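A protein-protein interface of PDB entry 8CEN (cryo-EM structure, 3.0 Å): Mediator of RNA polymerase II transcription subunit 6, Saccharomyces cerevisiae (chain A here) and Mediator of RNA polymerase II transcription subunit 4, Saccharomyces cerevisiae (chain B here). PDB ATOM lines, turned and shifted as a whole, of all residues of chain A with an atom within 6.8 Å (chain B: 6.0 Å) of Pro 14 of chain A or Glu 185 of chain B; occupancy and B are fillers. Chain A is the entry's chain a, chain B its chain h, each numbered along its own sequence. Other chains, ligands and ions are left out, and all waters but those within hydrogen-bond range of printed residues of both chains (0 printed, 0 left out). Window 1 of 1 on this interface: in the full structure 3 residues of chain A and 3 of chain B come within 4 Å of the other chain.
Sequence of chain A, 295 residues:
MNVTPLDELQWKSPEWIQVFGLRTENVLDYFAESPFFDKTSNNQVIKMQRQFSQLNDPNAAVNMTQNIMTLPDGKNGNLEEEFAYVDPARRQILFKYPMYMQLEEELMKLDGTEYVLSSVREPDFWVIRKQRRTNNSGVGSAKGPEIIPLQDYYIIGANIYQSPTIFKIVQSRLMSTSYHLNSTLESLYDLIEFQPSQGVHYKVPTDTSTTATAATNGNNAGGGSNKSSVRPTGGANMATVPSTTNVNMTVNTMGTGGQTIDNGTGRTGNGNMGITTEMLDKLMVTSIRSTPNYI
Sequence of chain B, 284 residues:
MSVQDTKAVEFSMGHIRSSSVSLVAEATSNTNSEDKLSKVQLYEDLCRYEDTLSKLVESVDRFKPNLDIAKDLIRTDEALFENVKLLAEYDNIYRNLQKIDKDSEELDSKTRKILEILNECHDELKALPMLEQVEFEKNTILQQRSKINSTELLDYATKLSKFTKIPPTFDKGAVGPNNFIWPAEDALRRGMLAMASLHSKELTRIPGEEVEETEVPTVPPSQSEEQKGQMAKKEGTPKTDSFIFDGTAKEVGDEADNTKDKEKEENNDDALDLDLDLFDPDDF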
ATOM      1  N   LYS A  12     -23.380  -8.346 -21.436  1.00  0.00           N
ATOM      2  CA  LYS A  12     -22.799  -9.629 -21.791  1.00  0.00           C
ATOM      3  C   LYS A  12     -23.918 -10.649 -21.925  1.00  0.00           C
ATOM      4  O   LYS A  12     -24.990 -10.496 -21.335  1.00  0.00           O
ATOM      5  CB  LYS A  12     -21.762 -10.102 -20.763  1.00  0.00           C
ATOM      6  CG  LYS A  12     -22.280 -10.303 -19.353  1.00  0.00           C
ATOM      7  CD  LYS A  12     -21.222 -10.982 -18.494  1.00  0.00           C
ATOM      8  CE  LYS A  12     -21.645 -11.073 -17.039  1.00  0.00           C
ATOM      9  NZ  LYS A  12     -21.474  -9.772 -16.337  1.00  0.00           N
ATOM     10  N   SER A  13     -23.658 -11.694 -22.713  1.00  0.00           N
ATOM     11  CA  SER A  13     -24.597 -12.798 -22.911  1.00  0.00           C
ATOM     12  C   SER A  13     -23.903 -14.085 -22.492  1.00  0.00           C
ATOM     13  O   SER A  13     -23.285 -14.770 -23.322  1.00  0.00           O
ATOM     14  CB  SER A  13     -25.068 -12.871 -24.362  1.00  0.00           C
ATOM     15  OG  SER A  13     -25.997 -13.927 -24.538  1.00  0.00           O
ATOM     16  N   PRO A  14     -23.962 -14.447 -21.210  1.00  0.00           N
ATOM     17  CA  PRO A  14     -23.283 -15.672 -20.771  1.00  0.00           C
ATOM     18  C   PRO A  14     -23.948 -16.954 -21.236  1.00  0.00           C
ATOM     19  O   PRO A  14     -23.289 -17.996 -21.207  1.00  0.00           O
ATOM     20  CB  PRO A  14     -23.288 -15.539 -19.243  1.00  0.00           C
ATOM     21  CG  PRO A  14     -23.330 -14.048 -19.041  1.00  0.00           C
ATOM     22  CD  PRO A  14     -24.337 -13.617 -20.057  1.00  0.00           C
ATOM     23  N   GLU A  15     -25.206 -16.921 -21.692  1.00  0.00           N
ATOM     24  CA  GLU A  15     -25.727 -18.063 -22.440  1.00  0.00           C
ATOM     25  C   GLU A  15     -24.929 -18.273 -23.719  1.00  0.00           C
ATOM     26  O   GLU A  15     -24.542 -19.402 -24.047  1.00  0.00           O
ATOM     27  CB  GLU A  15     -27.202 -17.864 -22.786  1.00  0.00           C
ATOM     28  CG  GLU A  15     -28.158 -17.847 -21.615  1.00  0.00           C
ATOM     29  CD  GLU A  15     -28.307 -16.471 -21.010  1.00  0.00           C
ATOM     30  OE1 GLU A  15     -27.691 -15.517 -21.529  1.00  0.00           O
ATOM     31  OE2 GLU A  15     -29.065 -16.342 -20.033  1.00  0.00           O
ATOM     32  N   TRP A  16     -24.662 -17.183 -24.442  1.00  0.00           N
ATOM     33  CA  TRP A  16     -23.828 -17.239 -25.635  1.00  0.00           C
ATOM     34  C   TRP A  16     -22.399 -17.639 -25.295  1.00  0.00           C
ATOM     35  O   TRP A  16     -21.752 -18.339 -26.079  1.00  0.00           O
ATOM     36  CB  TRP A  16     -23.871 -15.880 -26.337  1.00  0.00           C
ATOM     37  CG  TRP A  16     -23.445 -15.872 -27.770  1.00  0.00           C
ATOM     38  CD1 TRP A  16     -24.262 -15.878 -28.863  1.00  0.00           C
ATOM     39  CD2 TRP A  16     -22.107 -15.794 -28.271  1.00  0.00           C
ATOM     40  NE1 TRP A  16     -23.514 -15.839 -30.014  1.00  0.00           N
ATOM     41  CE2 TRP A  16     -22.188 -15.784 -29.676  1.00  0.00           C
ATOM     42  CE3 TRP A  16     -20.847 -15.746 -27.668  1.00  0.00           C
ATOM     43  CZ2 TRP A  16     -21.059 -15.728 -30.486  1.00  0.00           C
ATOM     44  CZ3 TRP A  16     -19.730 -15.689 -28.473  1.00  0.00           C
ATOM     45  CH2 TRP A  16     -19.843 -15.681 -29.867  1.00  0.00           C
ATOM     46  N   ILE A  17     -21.902 -17.223 -24.128  1.00  0.00           N
ATOM     47  CA  ILE A  17     -20.552 -17.599 -23.714  1.00  0.00           C
ATOM     48  C   ILE A  17     -20.477 -19.089 -23.387  1.00  0.00           C
ATOM     49  O   ILE A  17     -19.503 -19.766 -23.734  1.00  0.00           O
ATOM     50  CB  ILE A  17     -20.101 -16.721 -22.532  1.00  0.00           C
ATOM     51  CG1 ILE A  17     -20.043 -15.258 -22.966  1.00  0.00           C
ATOM     52  CG2 ILE A  17     -18.741 -17.157 -22.005  1.00  0.00           C
ATOM     53  CD1 ILE A  17     -19.176 -15.028 -24.182  1.00  0.00           C
ATOM     54  N   GLN A  18     -21.502 -19.626 -22.721  1.00  0.00           N
ATOM     55  CA  GLN A  18     -21.515 -21.050 -22.401  1.00  0.00           C
ATOM     56  C   GLN A  18     -21.693 -21.905 -23.651  1.00  0.00           C
ATOM     57  O   GLN A  18     -21.076 -22.970 -23.770  1.00  0.00           O
ATOM     58  CB  GLN A  18     -22.613 -21.356 -21.382  1.00  0.00           C
ATOM     59  CG  GLN A  18     -22.357 -20.868 -19.948  1.00  0.00           C
ATOM     60  CD  GLN A  18     -21.006 -21.286 -19.378  1.00  0.00           C
ATOM     61  OE1 GLN A  18     -19.985 -20.635 -19.607  1.00  0.00           O
ATOM     62  NE2 GLN A  18     -21.001 -22.383 -18.630  1.00  0.00           N
ATOM     63  N   VAL A  19     -22.525 -21.463 -24.594  1.00  0.00           N
ATOM     64  CA  VAL A  19     -22.784 -22.272 -25.783  1.00  0.00           C
ATOM     65  C   VAL A  19     -21.645 -22.144 -26.788  1.00  0.00           C
ATOM     66  O   VAL A  19     -20.978 -23.131 -27.124  1.00  0.00           O
ATOM     67  CB  VAL A  19     -24.137 -21.892 -26.411  1.00  0.00           C
ATOM     68  CG1 VAL A  19     -24.311 -22.580 -27.754  1.00  0.00           C
ATOM     69  CG2 VAL A  19     -25.275 -22.271 -25.477  1.00  0.00           C
ATOM     70  N   TYR A  30     -20.935 -11.982 -31.723  1.00  0.00           N
ATOM     71  CA  TYR A  30     -21.263 -11.821 -30.309  1.00  0.00           C
ATOM     72  C   TYR A  30     -21.815 -10.428 -30.041  1.00  0.00           C
ATOM     73  O   TYR A  30     -22.798 -10.268 -29.308  1.00  0.00           O
ATOM     74  CB  TYR A  30     -20.025 -12.076 -29.453  1.00  0.00           C
ATOM     75  CG  TYR A  30     -20.213 -11.800 -27.979  1.00  0.00           C
ATOM     76  CD1 TYR A  30     -21.276 -12.351 -27.276  1.00  0.00           C
ATOM     77  CD2 TYR A  30     -19.322 -10.989 -27.288  1.00  0.00           C
ATOM     78  CE1 TYR A  30     -21.445 -12.105 -25.929  1.00  0.00           C
ATOM     79  CE2 TYR A  30     -19.484 -10.737 -25.942  1.00  0.00           C
ATOM     80  CZ  TYR A  30     -20.548 -11.296 -25.269  1.00  0.00           C
ATOM     81  OH  TYR A  30     -20.710 -11.047 -23.929  1.00  0.00           O
ATOM     82  N   ALA A 158     -15.468 -10.487 -22.507  1.00  0.00           N
ATOM     83  CA  ALA A 158     -16.797 -10.724 -23.072  1.00  0.00           C
ATOM     84  C   ALA A 158     -17.865  -9.815 -22.472  1.00  0.00           C
ATOM     85  O   ALA A 158     -19.056 -10.124 -22.543  1.00  0.00           O
ATOM     86  CB  ALA A 158     -17.218 -12.191 -22.935  1.00  0.00           C
ATOM     87  N   ASN B 178     -16.101 -20.026 -10.960  1.00  0.00           N
ATOM     88  CA  ASN B 178     -17.374 -19.436 -11.362  1.00  0.00           C
ATOM     89  C   ASN B 178     -18.568 -20.210 -10.824  1.00  0.00           C
ATOM     90  O   ASN B 178     -19.557 -19.604 -10.402  1.00  0.00           O
ATOM     91  CB  ASN B 178     -17.438 -19.350 -12.881  1.00  0.00           C
ATOM     92  CG  ASN B 178     -16.518 -18.296 -13.425  1.00  0.00           C
ATOM     93  OD1 ASN B 178     -15.409 -18.597 -13.863  1.00  0.00           O
ATOM     94  ND2 ASN B 178     -16.962 -17.045 -13.388  1.00  0.00           N
ATOM     95  N   ASN B 179     -18.516 -21.541 -10.853  1.00  0.00           N
ATOM     96  CA  ASN B 179     -19.631 -22.355 -10.381  1.00  0.00           C
ATOM     97  C   ASN B 179     -19.215 -23.321  -9.280  1.00  0.00           C
ATOM     98  O   ASN B 179     -19.880 -24.339  -9.066  1.00  0.00           O
ATOM     99  CB  ASN B 179     -20.275 -23.110 -11.541  1.00  0.00           C
ATOM    100  CG  ASN B 179     -21.068 -22.200 -12.457  1.00  0.00           C
ATOM    101  OD1 ASN B 179     -22.225 -21.892 -12.187  1.00  0.00           O
ATOM    102  ND2 ASN B 179     -20.447 -21.768 -13.548  1.00  0.00           N
ATOM    103  N   PRO B 183     -22.865 -19.632  -7.322  1.00  0.00           N
ATOM    104  CA  PRO B 183     -23.523 -19.800  -8.624  1.00  0.00           C
ATOM    105  C   PRO B 183     -23.187 -18.629  -9.536  1.00  0.00           C
ATOM    106  O   PRO B 183     -23.307 -17.465  -9.147  1.00  0.00           O
ATOM    107  CB  PRO B 183     -25.014 -19.831  -8.272  1.00  0.00           C
ATOM    108  CG  PRO B 183     -25.111 -19.145  -6.966  1.00  0.00           C
ATOM    109  CD  PRO B 183     -23.838 -19.434  -6.236  1.00  0.00           C
ATOM    110  N   ALA B 184     -22.757 -18.944 -10.754  1.00  0.00           N
ATOM    111  CA  ALA B 184     -22.356 -17.917 -11.700  1.00  0.00           C
ATOM    112  C   ALA B 184     -23.583 -17.219 -12.279  1.00  0.00           C
ATOM    113  O   ALA B 184     -24.733 -17.552 -11.967  1.00  0.00           O
ATOM    114  CB  ALA B 184     -21.497 -18.519 -12.808  1.00  0.00           C
ATOM    115  N   GLU B 185     -23.323 -16.228 -13.138  1.00  0.00           N
ATOM    116  CA  GLU B 185     -24.406 -15.502 -13.792  1.00  0.00           C
ATOM    117  C   GLU B 185     -25.246 -16.434 -14.648  1.00  0.00           C
ATOM    118  O   GLU B 185     -26.478 -16.410 -14.574  1.00  0.00           O
ATOM    119  CB  GLU B 185     -23.847 -14.359 -14.641  1.00  0.00           C
ATOM    120  CG  GLU B 185     -24.856 -13.249 -14.938  1.00  0.00           C
ATOM    121  CD  GLU B 185     -25.690 -13.498 -16.193  1.00  0.00           C
ATOM    122  OE1 GLU B 185     -25.501 -14.527 -16.863  1.00  0.00           O
ATOM    123  OE2 GLU B 185     -26.559 -12.667 -16.513  1.00  0.00           O
ATOM    124  N   ASP B 186     -24.593 -17.251 -15.482  1.00  0.00           N
ATOM    125  CA  ASP B 186     -25.324 -18.181 -16.336  1.00  0.00           C
ATOM    126  C   ASP B 186     -26.090 -19.203 -15.513  1.00  0.00           C
ATOM    127  O   ASP B 186     -27.175 -19.633 -15.918  1.00  0.00           O
ATOM    128  CB  ASP B 186     -24.367 -18.885 -17.297  1.00  0.00           C
ATOM    129  CG  ASP B 186     -23.137 -19.427 -16.599  1.00  0.00           C
ATOM    130  OD1 ASP B 186     -22.408 -18.626 -15.980  1.00  0.00           O
ATOM    131  OD2 ASP B 186     -22.902 -20.652 -16.666  1.00  0.00           O
ATOM    132  N   ALA B 187     -25.549 -19.585 -14.353  1.00  0.00           N
ATOM    133  CA  ALA B 187     -26.274 -20.457 -13.436  1.00  0.00           C
ATOM    134  C   ALA B 187     -27.540 -19.788 -12.923  1.00  0.00           C
ATOM    135  O   ALA B 187     -28.592 -20.428 -12.836  1.00  0.00           O
ATOM    136  CB  ALA B 187     -25.374 -20.860 -12.270  1.00  0.00           C
ATOM    137  N   LEU B 188     -27.465 -18.496 -12.588  1.00  0.00           N
ATOM    138  CA  LEU B 188     -28.664 -17.799 -12.128  1.00  0.00           C
ATOM    139  C   LEU B 188     -29.663 -17.569 -13.258  1.00  0.00           C
ATOM    140  O   LEU B 188     -30.872 -17.511 -13.010  1.00  0.00           O
ATOM    141  CB  LEU B 188     -28.286 -16.472 -11.468  1.00  0.00           C
ATOM    142  CG  LEU B 188     -27.360 -16.587 -10.257  1.00  0.00           C
ATOM    143  CD1 LEU B 188     -26.917 -15.219  -9.766  1.00  0.00           C
ATOM    144  CD2 LEU B 188     -28.037 -17.369  -9.146  1.00  0.00           C
ATOM    145  N   ARG B 189     -29.182 -17.434 -14.496  1.00  0.00           N
ATOM    146  CA  ARG B 189     -30.084 -17.261 -15.633  1.00  0.00           C
ATOM    147  C   ARG B 189     -30.820 -18.555 -15.958  1.00  0.00           C
ATOM    148  O   ARG B 189     -32.056 -18.590 -15.983  1.00  0.00           O
ATOM    149  CB  ARG B 189     -29.316 -16.781 -16.862  1.00  0.00           C
ATOM    150  CG  ARG B 189     -28.577 -15.480 -16.701  1.00  0.00           C
ATOM    151  CD  ARG B 189     -29.470 -14.257 -16.806  1.00  0.00           C
ATOM    152  NE  ARG B 189     -29.762 -13.888 -18.188  1.00  0.00           N
ATOM    153  CZ  ARG B 189     -28.885 -13.417 -19.067  1.00  0.00           C
ATOM    154  NH1 ARG B 189     -27.615 -13.217 -18.751  1.00  0.00           N
ATOM    155  NH2 ARG B 189     -29.295 -13.136 -20.300  1.00  0.00           N
ATOM    156  N   ARG B 190     -30.075 -19.634 -16.226  1.00  0.00           N
ATOM    157  CA  ARG B 190     -30.712 -20.909 -16.538  1.00  0.00           C
ATOM    158  C   ARG B 190     -31.373 -21.534 -15.322  1.00  0.00           C
ATOM    159  O   ARG B 190     -32.155 -22.478 -15.477  1.00  0.00           O
ATOM    160  CB  ARG B 190     -29.709 -21.906 -17.120  1.00  0.00           C
ATOM    161  CG  ARG B 190     -28.697 -22.426 -16.117  1.00  0.00           C
ATOM    162  CD  ARG B 190     -27.725 -23.400 -16.755  1.00  0.00           C
ATOM    163  NE  ARG B 190     -26.780 -23.930 -15.781  1.00  0.00           N
ATOM    164  CZ  ARG B 190     -25.599 -23.390 -15.514  1.00  0.00           C
ATOM    165  NH1 ARG B 190     -25.174 -22.310 -16.148  1.00  0.00           N
ATOM    166  NH2 ARG B 190     -24.823 -23.950 -14.590  1.00  0.00           N
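Of the 10 printed residues of chain A, 3 touch a printed residue of chain B.
Along chain A the printed residues that touch a printed residue of chain B span positions 14 to 18.
Of the 10 printed residues of chain B, 3 touch a printed residue of chain A.
Printed residues of chain B within 4 Å of Pro 14 of chain A: Glu 185 (3.1 Å) and Arg 189 (3.6 Å).
Of the printed residues of chain B, Gln 18 of chain A touches Asp 186 (3.2 Å).
Tyr 30 of chain A touches none of the printed residues of chain B.
Ala 158 of chain A touches none of the printed residues of chain B.
Printed residues of chain A within 4 Å of Asp 186 of chain B: Gln 18 (3.2 Å).
Of the printed residues of chain A, Arg 189 of chain B touches Pro 14 (3.6 Å) and Glu 15 (3.1 Å).
The nearest residue of chain A that does not touch Glu 185 of chain B is Lys 12 of chain A (4.4 Å).
Glu 185 of chain B touches Pro 14 of chain A.
Arg 189 of chain B touches Pro 14 of chain A (NH1 to CD, 3.6 Å).
OE1 of Glu 15 of chain A lies within salt-bridge range of NH2 of Arg 189 of chain B, at 3.1 Å.
NE2 of Gln 18 of chain A lies within hydrogen-bond range of OD2 of Asp 186 of chain B (3.2 Å).
OE2 of Glu 185 of chain B is in salt-bridge range of NH1 of Arg 189 of chain B (2.5 Å).
The side-chain carboxylate of Asp 186 of chain B lies within salt-bridge range of the guanidinium group of Arg 190 of chain B.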
